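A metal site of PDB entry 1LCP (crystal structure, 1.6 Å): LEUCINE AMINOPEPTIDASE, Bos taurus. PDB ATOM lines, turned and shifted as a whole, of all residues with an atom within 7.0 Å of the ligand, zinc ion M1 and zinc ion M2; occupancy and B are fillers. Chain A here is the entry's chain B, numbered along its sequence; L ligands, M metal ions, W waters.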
ATOM      1  N   LYS A 250       8.712  11.862   8.510  1.00  0.00           N
ATOM      2  CA  LYS A 250       9.111  11.146   7.292  1.00  0.00           C
ATOM      3  C   LYS A 250       8.048  11.373   6.184  1.00  0.00           C
ATOM      4  O   LYS A 250       6.869  11.027   6.375  1.00  0.00           O
ATOM      5  CB  LYS A 250       9.258   9.648   7.590  1.00  0.00           C
ATOM      6  CG  LYS A 250       9.380   8.770   6.358  1.00  0.00           C
ATOM      7  CD  LYS A 250       9.459   7.283   6.729  1.00  0.00           C
ATOM      8  CE  LYS A 250       9.390   6.396   5.475  1.00  0.00           C
ATOM      9  NZ  LYS A 250       9.471   4.930   5.763  1.00  0.00           N
ATOM     10  N   ILE A 252       7.742  10.150   2.711  1.00  0.00           N
ATOM     11  CA  ILE A 252       7.882   9.382   1.472  1.00  0.00           C
ATOM     12  C   ILE A 252       6.485   9.299   0.856  1.00  0.00           C
ATOM     13  O   ILE A 252       5.622   8.587   1.380  1.00  0.00           O
ATOM     14  CB  ILE A 252       8.460   7.955   1.725  1.00  0.00           C
ATOM     15  CG1 ILE A 252       9.895   8.037   2.272  1.00  0.00           C
ATOM     16  CG2 ILE A 252       8.423   7.125   0.438  1.00  0.00           C
ATOM     17  CD1 ILE A 252      10.898   8.655   1.284  1.00  0.00           C
ATOM     18  N   ASP A 255       6.467   4.630  -1.566  1.00  0.00           N
ATOM     19  CA  ASP A 255       7.631   3.783  -1.342  1.00  0.00           C
ATOM     20  C   ASP A 255       7.523   2.461  -2.091  1.00  0.00           C
ATOM     21  O   ASP A 255       6.805   1.557  -1.659  1.00  0.00           O
ATOM     22  CB  ASP A 255       7.808   3.510   0.168  1.00  0.00           C
ATOM     23  CG  ASP A 255       9.104   2.745   0.497  1.00  0.00           C
ATOM     24  OD1 ASP A 255       9.990   2.636  -0.384  1.00  0.00           O
ATOM     25  OD2 ASP A 255       9.243   2.282   1.654  1.00  0.00           O
ATOM     26  N   SER A 256       8.231   2.340  -3.214  1.00  0.00           N
ATOM     27  CA  SER A 256       8.251   1.100  -3.997  1.00  0.00           C
ATOM     28  C   SER A 256       9.414   0.215  -3.541  1.00  0.00           C
ATOM     29  O   SER A 256       9.554  -0.931  -4.004  1.00  0.00           O
ATOM     30  CB  SER A 256       8.484   1.416  -5.488  1.00  0.00           C
ATOM     31  OG  SER A 256       9.857   1.740  -5.707  1.00  0.00           O
ATOM     32  N   GLY A 257      10.302   0.792  -2.734  1.00  0.00           N
ATOM     33  CA  GLY A 257      11.491   0.099  -2.264  1.00  0.00           C
ATOM     34  C   GLY A 257      12.747   0.423  -3.081  1.00  0.00           C
ATOM     35  O   GLY A 257      13.867   0.254  -2.589  1.00  0.00           O
ATOM     36  N   GLY A 258      12.553   0.945  -4.298  1.00  0.00           N
ATOM     37  CA  GLY A 258      13.681   1.259  -5.159  1.00  0.00           C
ATOM     38  C   GLY A 258      14.252  -0.029  -5.747  1.00  0.00           C
ATOM     39  O   GLY A 258      13.492  -0.950  -6.053  1.00  0.00           O
ATOM     40  N   SER A 260      15.901  -2.321  -4.282  1.00  0.00           N
ATOM     41  CA  SER A 260      15.598  -3.398  -3.338  1.00  0.00           C
ATOM     42  C   SER A 260      14.057  -3.352  -3.311  1.00  0.00           C
ATOM     43  O   SER A 260      13.432  -3.077  -2.278  1.00  0.00           O
ATOM     44  CB  SER A 260      16.161  -3.067  -1.947  1.00  0.00           C
ATOM     45  OG  SER A 260      17.559  -2.784  -1.989  1.00  0.00           O
ATOM     46  N   LYS A 262       9.965  -3.771  -3.442  1.00  0.00           N
ATOM     47  CA  LYS A 262       8.971  -4.417  -2.576  1.00  0.00           C
ATOM     48  C   LYS A 262       8.140  -5.466  -3.321  1.00  0.00           C
ATOM     49  O   LYS A 262       8.095  -5.471  -4.556  1.00  0.00           O
ATOM     50  CB  LYS A 262       7.985  -3.374  -2.049  1.00  0.00           C
ATOM     51  CG  LYS A 262       8.512  -2.469  -0.958  1.00  0.00           C
ATOM     52  CD  LYS A 262       7.406  -1.552  -0.428  1.00  0.00           C
ATOM     53  CE  LYS A 262       7.949  -0.628   0.640  1.00  0.00           C
ATOM     54  NZ  LYS A 262       8.525  -1.382   1.785  1.00  0.00           N
ATOM     55  N   MET A 270       1.540   1.933   0.539  1.00  0.00           N
ATOM     56  CA  MET A 270       2.744   2.740   0.633  1.00  0.00           C
ATOM     57  C   MET A 270       2.537   4.212   0.210  1.00  0.00           C
ATOM     58  O   MET A 270       3.451   5.034   0.286  1.00  0.00           O
ATOM     59  CB  MET A 270       3.907   2.060  -0.096  1.00  0.00           C
ATOM     60  CG  MET A 270       4.353   0.740   0.568  1.00  0.00           C
ATOM     61  SD  MET A 270       4.847   0.948   2.323  1.00  0.00           S
ATOM     62  CE  MET A 270       3.364   0.430   3.192  1.00  0.00           C
ATOM     63  N   ASP A 273       3.188   6.310   3.189  1.00  0.00           N
ATOM     64  CA  ASP A 273       4.524   6.316   3.791  1.00  0.00           C
ATOM     65  C   ASP A 273       4.954   7.749   4.165  1.00  0.00           C
ATOM     66  O   ASP A 273       6.102   7.988   4.576  1.00  0.00           O
ATOM     67  CB  ASP A 273       5.538   5.640   2.857  1.00  0.00           C
ATOM     68  CG  ASP A 273       6.701   4.992   3.614  1.00  0.00           C
ATOM     69  OD1 ASP A 273       6.556   4.633   4.807  1.00  0.00           O
ATOM     70  OD2 ASP A 273       7.782   4.827   3.005  1.00  0.00           O
ATOM     71  N   ASN A 305      10.332   7.043  -3.550  1.00  0.00           N
ATOM     72  CA  ASN A 305      11.421   6.060  -3.562  1.00  0.00           C
ATOM     73  C   ASN A 305      11.080   5.116  -4.730  1.00  0.00           C
ATOM     74  O   ASN A 305      10.223   4.223  -4.588  1.00  0.00           O
ATOM     75  CB  ASN A 305      11.505   5.291  -2.222  1.00  0.00           C
ATOM     76  CG  ASN A 305      12.733   4.372  -2.117  1.00  0.00           C
ATOM     77  OD1 ASN A 305      12.712   3.367  -1.408  1.00  0.00           O
ATOM     78  ND2 ASN A 305      13.817   4.726  -2.805  1.00  0.00           N
ATOM     79  N   ASN A 330      20.398  -1.662   1.796  1.00  0.00           N
ATOM     80  CA  ASN A 330      19.060  -1.951   1.294  1.00  0.00           C
ATOM     81  C   ASN A 330      18.371  -0.619   1.001  1.00  0.00           C
ATOM     82  O   ASN A 330      18.110   0.182   1.914  1.00  0.00           O
ATOM     83  CB  ASN A 330      18.257  -2.754   2.340  1.00  0.00           C
ATOM     84  CG  ASN A 330      16.957  -3.325   1.775  1.00  0.00           C
ATOM     85  OD1 ASN A 330      16.730  -4.536   1.786  1.00  0.00           O
ATOM     86  ND2 ASN A 330      16.075  -2.454   1.335  1.00  0.00           N
ATOM     87  N   THR A 331      18.049  -0.384  -0.269  1.00  0.00           N
ATOM     88  CA  THR A 331      17.434   0.869  -0.687  1.00  0.00           C
ATOM     89  C   THR A 331      16.015   1.118  -0.137  1.00  0.00           C
ATOM     90  O   THR A 331      15.506   2.242  -0.219  1.00  0.00           O
ATOM     91  CB  THR A 331      17.446   1.015  -2.245  1.00  0.00           C
ATOM     92  OG1 THR A 331      16.569   0.043  -2.838  1.00  0.00           O
ATOM     93  CG2 THR A 331      18.847   0.782  -2.794  1.00  0.00           C
ATOM     94  N   ASP A 332      15.377   0.058   0.379  1.00  0.00           N
ATOM     95  CA  ASP A 332      14.030   0.111   0.943  1.00  0.00           C
ATOM     96  C   ASP A 332      14.032   0.566   2.421  1.00  0.00           C
ATOM     97  O   ASP A 332      12.972   0.685   3.058  1.00  0.00           O
ATOM     98  CB  ASP A 332      13.316  -1.248   0.751  1.00  0.00           C
ATOM     99  CG  ASP A 332      11.788  -1.160   0.893  1.00  0.00           C
ATOM    100  OD1 ASP A 332      11.210  -0.044   0.873  1.00  0.00           O
ATOM    101  OD2 ASP A 332      11.172  -2.232   1.020  1.00  0.00           O
ATOM    102  N   ALA A 333      15.215   0.751   2.993  1.00  0.00           N
ATOM    103  CA  ALA A 333      15.330   1.271   4.363  1.00  0.00           C
ATOM    104  C   ALA A 333      15.627   2.763   4.093  1.00  0.00           C
ATOM    105  O   ALA A 333      16.630   3.317   4.566  1.00  0.00           O
ATOM    106  CB  ALA A 333      16.491   0.615   5.125  1.00  0.00           C
ATOM    107  N   GLU A 334      14.726   3.412   3.353  1.00  0.00           N
ATOM    108  CA  GLU A 334      14.911   4.803   2.954  1.00  0.00           C
ATOM    109  C   GLU A 334      14.454   5.861   3.952  1.00  0.00           C
ATOM    110  O   GLU A 334      14.927   7.002   3.931  1.00  0.00           O
ATOM    111  CB  GLU A 334      14.235   5.039   1.581  1.00  0.00           C
ATOM    112  CG  GLU A 334      12.735   5.379   1.619  1.00  0.00           C
ATOM    113  CD  GLU A 334      11.848   4.271   2.205  1.00  0.00           C
ATOM    114  OE1 GLU A 334      12.125   3.067   1.990  1.00  0.00           O
ATOM    115  OE2 GLU A 334      10.849   4.626   2.864  1.00  0.00           O
ATOM    116  N   GLY A 335      13.512   5.501   4.821  1.00  0.00           N
ATOM    117  CA  GLY A 335      13.034   6.471   5.802  1.00  0.00           C
ATOM    118  C   GLY A 335      14.136   6.990   6.707  1.00  0.00           C
ATOM    119  O   GLY A 335      14.222   8.195   6.954  1.00  0.00           O
ATOM    120  N   ARG A 336      15.001   6.097   7.184  1.00  0.00           N
ATOM    121  CA  ARG A 336      16.080   6.515   8.069  1.00  0.00           C
ATOM    122  C   ARG A 336      17.101   7.369   7.324  1.00  0.00           C
ATOM    123  O   ARG A 336      17.743   8.254   7.905  1.00  0.00           O
ATOM    124  CB  ARG A 336      16.711   5.321   8.791  1.00  0.00           C
ATOM    125  CG  ARG A 336      17.453   4.349   7.900  1.00  0.00           C
ATOM    126  CD  ARG A 336      17.707   3.008   8.619  1.00  0.00           C
ATOM    127  NE  ARG A 336      16.507   2.162   8.619  1.00  0.00           N
ATOM    128  CZ  ARG A 336      16.420   0.973   9.215  1.00  0.00           C
ATOM    129  NH1 ARG A 336      17.441   0.484   9.908  1.00  0.00           N
ATOM    130  NH2 ARG A 336      15.283   0.288   9.131  1.00  0.00           N
ATOM    131  N   THR A 359       6.490   6.266   9.589  1.00  0.00           N
ATOM    132  CA  THR A 359       5.939   4.922   9.321  1.00  0.00           C
ATOM    133  C   THR A 359       7.245   4.186   8.967  1.00  0.00           C
ATOM    134  O   THR A 359       7.466   3.780   7.828  1.00  0.00           O
ATOM    135  CB  THR A 359       5.006   4.961   8.083  1.00  0.00           C
ATOM    136  OG1 THR A 359       5.578   5.822   7.090  1.00  0.00           O
ATOM    137  CG2 THR A 359       3.637   5.491   8.466  1.00  0.00           C
ATOM    138  N   LEU A 360       8.095   4.026   9.972  1.00  0.00           N
ATOM    139  CA  LEU A 360       9.434   3.490   9.767  1.00  0.00           C
ATOM    140  C   LEU A 360       9.708   2.020   9.502  1.00  0.00           C
ATOM    141  O   LEU A 360      10.513   1.701   8.617  1.00  0.00           O
ATOM    142  CB  LEU A 360      10.356   3.989  10.891  1.00  0.00           C
ATOM    143  CG  LEU A 360      11.853   4.100  10.558  1.00  0.00           C
ATOM    144  CD1 LEU A 360      12.079   5.156   9.451  1.00  0.00           C
ATOM    145  CD2 LEU A 360      12.660   4.462  11.808  1.00  0.00           C
ATOM    146  N   THR A 361       9.106   1.131  10.278  1.00  0.00           N
ATOM    147  CA  THR A 361       9.402  -0.284  10.074  1.00  0.00           C
ATOM    148  C   THR A 361       8.230  -1.244  10.132  1.00  0.00           C
ATOM    149  O   THR A 361       7.301  -1.071  10.927  1.00  0.00           O
ATOM    150  CB  THR A 361      10.416  -0.799  11.157  1.00  0.00           C
ATOM    151  OG1 THR A 361       9.824  -0.711  12.466  1.00  0.00           O
ATOM    152  CG2 THR A 361      11.705   0.019  11.141  1.00  0.00           C
ATOM    153  N   GLY A 362       8.294  -2.285   9.301  1.00  0.00           N
ATOM    154  CA  GLY A 362       7.277  -3.310   9.343  1.00  0.00           C
ATOM    155  C   GLY A 362       7.427  -4.049  10.678  1.00  0.00           C
ATOM    156  O   GLY A 362       6.463  -4.600  11.218  1.00  0.00           O
ATOM    157  N   ALA A 363       8.640  -4.029  11.222  1.00  0.00           N
ATOM    158  CA  ALA A 363       8.931  -4.680  12.496  1.00  0.00           C
ATOM    159  C   ALA A 363       8.084  -4.112  13.626  1.00  0.00           C
ATOM    160  O   ALA A 363       7.653  -4.851  14.515  1.00  0.00           O
ATOM    161  CB  ALA A 363      10.412  -4.574  12.842  1.00  0.00           C
ATOM    162  N   ASP A 365       5.076  -3.041  13.362  1.00  0.00           N
ATOM    163  CA  ASP A 365       3.749  -3.625  13.202  1.00  0.00           C
ATOM    164  C   ASP A 365       3.731  -5.042  13.796  1.00  0.00           C
ATOM    165  O   ASP A 365       2.782  -5.438  14.501  1.00  0.00           O
ATOM    166  CB  ASP A 365       3.360  -3.672  11.715  1.00  0.00           C
ATOM    167  CG  ASP A 365       1.958  -4.175  11.504  1.00  0.00           C
ATOM    168  OD1 ASP A 365       1.039  -3.600  12.103  1.00  0.00           O
ATOM    169  OD2 ASP A 365       1.779  -5.184  10.799  1.00  0.00           O
ATOM    170  N   ASP A 449       7.464   5.541  16.024  1.00  0.00           N
ATOM    171  CA  ASP A 449       7.334   4.666  14.867  1.00  0.00           C
ATOM    172  C   ASP A 449       5.844   4.357  14.793  1.00  0.00           C
ATOM    173  O   ASP A 449       5.307   3.597  15.610  1.00  0.00           O
ATOM    174  CB  ASP A 449       8.189   3.381  15.019  1.00  0.00           C
ATOM    175  CG  ASP A 449       8.272   2.537  13.731  1.00  0.00           C
ATOM    176  OD1 ASP A 449       7.380   2.654  12.856  1.00  0.00           O
ATOM    177  OD2 ASP A 449       9.240   1.740  13.592  1.00  0.00           O
ATOM    178  N   ILE A 450       5.167   4.961  13.818  1.00  0.00           N
ATOM    179  CA  ILE A 450       3.722   4.815  13.636  1.00  0.00           C
ATOM    180  C   ILE A 450       3.307   3.833  12.535  1.00  0.00           C
ATOM    181  O   ILE A 450       2.142   3.819  12.118  1.00  0.00           O
ATOM    182  CB  ILE A 450       3.071   6.205  13.356  1.00  0.00           C
ATOM    183  CG1 ILE A 450       3.576   6.767  12.015  1.00  0.00           C
ATOM    184  CG2 ILE A 450       3.399   7.191  14.510  1.00  0.00           C
ATOM    185  CD1 ILE A 450       2.819   7.984  11.545  1.00  0.00           C
ATOM    186  N   ALA A 451       4.234   2.999  12.080  1.00  0.00           N
ATOM    187  CA  ALA A 451       3.939   2.032  11.008  1.00  0.00           C
ATOM    188  C   ALA A 451       2.746   1.119  11.317  1.00  0.00           C
ATOM    189  O   ALA A 451       1.946   0.809  10.433  1.00  0.00           O
ATOM    190  CB  ALA A 451       5.175   1.192  10.692  1.00  0.00           C
ATOM    191  N   GLY A 452       2.642   0.667  12.566  1.00  0.00           N
ATOM    192  CA  GLY A 452       1.545  -0.218  12.954  1.00  0.00           C
ATOM    193  C   GLY A 452       0.184   0.456  13.087  1.00  0.00           C
ATOM    194  O   GLY A 452      -0.843  -0.221  13.036  1.00  0.00           O
ATOM    195  N   MET A 454      -0.787   2.947  11.005  1.00  0.00           N
ATOM    196  CA  MET A 454      -1.015   3.620   9.731  1.00  0.00           C
ATOM    197  C   MET A 454      -2.448   3.451   9.236  1.00  0.00           C
ATOM    198  O   MET A 454      -3.044   4.389   8.692  1.00  0.00           O
ATOM    199  CB  MET A 454      -0.018   3.088   8.675  1.00  0.00           C
ATOM    200  CG  MET A 454       0.157   3.975   7.446  1.00  0.00           C
ATOM    201  SD  MET A 454       1.418   3.320   6.319  1.00  0.00           S
ATOM    202  CE  MET A 454       0.532   1.916   5.612  1.00  0.00           C
HETATM  203  C1  LIG L   1       8.429   1.203   5.433  1.00  0.00           C
HETATM  204  C2  LIG L   1       7.644  -0.131   5.457  1.00  0.00           C
HETATM  205  C3  LIG L   1       6.166  -0.040   5.879  1.00  0.00           C
HETATM  206  C4  LIG L   1       5.993   0.596   7.243  1.00  0.00           C
HETATM  207  C5  LIG L   1       5.470  -1.408   5.878  1.00  0.00           C
HETATM  208  N1  LIG L   1       7.816   2.115   4.462  1.00  0.00           N
HETATM  209  P1  LIG L   1      10.145   0.842   4.900  1.00  0.00           P
HETATM  210  O1  LIG L   1      10.819   2.218   4.650  1.00  0.00           O
HETATM  211  O2  LIG L   1      10.062   0.059   3.536  1.00  0.00           O
HETATM  212  O3  LIG L   1      10.857   0.040   6.030  1.00  0.00           O
HETATM  213 ZN    ZN M   1      11.054   1.373   2.281  1.00  0.00          ZN
HETATM  214 ZN    ZN M   2       9.311   3.713   3.982  1.00  0.00          ZN
HETATM  215  O   HOH W   1       7.675  -4.079   5.614  1.00  0.00           O
HETATM  216  O   HOH W   2      13.181   0.648   7.042  1.00  0.00           O
HETATM  217  O   HOH W   3      10.083  -2.337   7.148  1.00  0.00           O
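The backbone NH (N) of Asp 332 is in hydrogen-bond range of the backbone carbonyl oxygen (O) of Gly 257, 3.3 Å away. The backbone NH of Asp 332 lies close to the side-chain amide nitrogen of Asn 330 (2.8 Å). The side-chain carboxylate (OD2) of Asp 255 lies close to the side-chain amino group (NZ) of Lys 262, at 3.7 Å. OD1 of Asp 273 is in hydrogen-bond range of OG1 of Thr 359, 2.8 Å away. The backbone carbonyl oxygen (O) of Asp 273 lies within hydrogen-bond range of the backbone NH (N) of Ile 252 (3.3 Å). O of Ser 256 is in hydrogen-bond range of N of Lys 262 (2.9 Å). N of Leu 360 lies within hydrogen-bond range of OD1 of Asp 449. The backbone NH of Ala 451 lies within hydrogen-bond range of the side-chain carboxylate of Asp 449, 3.3 Å away.
Zinc ion M2 is bound by the side-chain carboxylate (OE2) of Glu 334 (2.1 Å), the side-chain carboxylate (OD2) of Asp 273 (2.1 Å), the side-chain amino group (NZ) of Lys 250 (2.2 Å), an oxygen (O1) of the ligand (2.2 Å) and a nitrogen (N1) of the ligand (2.2 Å). Slightly farther from zinc ion M2 lies the side-chain carboxylate (OD2) of Asp 255 (2.7 Å).
Four residues have an atom within 4 Å of zinc ion M2: Lys 250, Asp 255, Asp 273 and Glu 334. The nearest printed residue that does not touch zinc ion M2 is Thr 359 (4.3 Å).
Zinc ion M1 is bound by the side-chain carboxylate of Asp 332 (2.0 Å), the side-chain carboxylate of Glu 334 (2.0 Å), an oxygen (O2) of the ligand (2.1 Å), the side-chain carboxylate of Asp 255 (2.1 Å), the backbone carbonyl oxygen of Asp 332 (2.2 Å) and an oxygen (O1) of the ligand (2.5 Å). Zinc ion M1 has six donor atoms within binding distance.
The side-chain amino group (NZ) of Lys 262 sits close to an oxygen (O2) of the ligand, 2.7 Å away. An oxygen (O3) of the ligand sits close to the backbone carbonyl oxygen (O) of Leu 360 (3.1 Å).
Water W2 lies within hydrogen-bond range of O3 of the ligand, NH2 of Arg 336 and O of Leu 360. Water W3 lies within hydrogen-bond range of an oxygen (O3) of the ligand and the backbone NH of Gly 362.
Lys 262 touches zinc ion M1 (NZ to ZN, 3.8 Å). Of the 29 residues printed, 4 come within 4 Å of zinc ion M1.
Met 270 touches the ligand. O of Thr 359 touches C4 of the ligand, at 3.6 Å. Ala 451 touches the ligand (CB to C4, 3.6 Å). Hydrophobic or aromatic side chains that line the ligand: Met 270 and Ala 451. Within 4 Å of the ligand: Lys 250, Asp 255, Lys 262, Met 270, Asp 273, Asp 332, Glu 334, Thr 359, Leu 360 and Ala 451.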
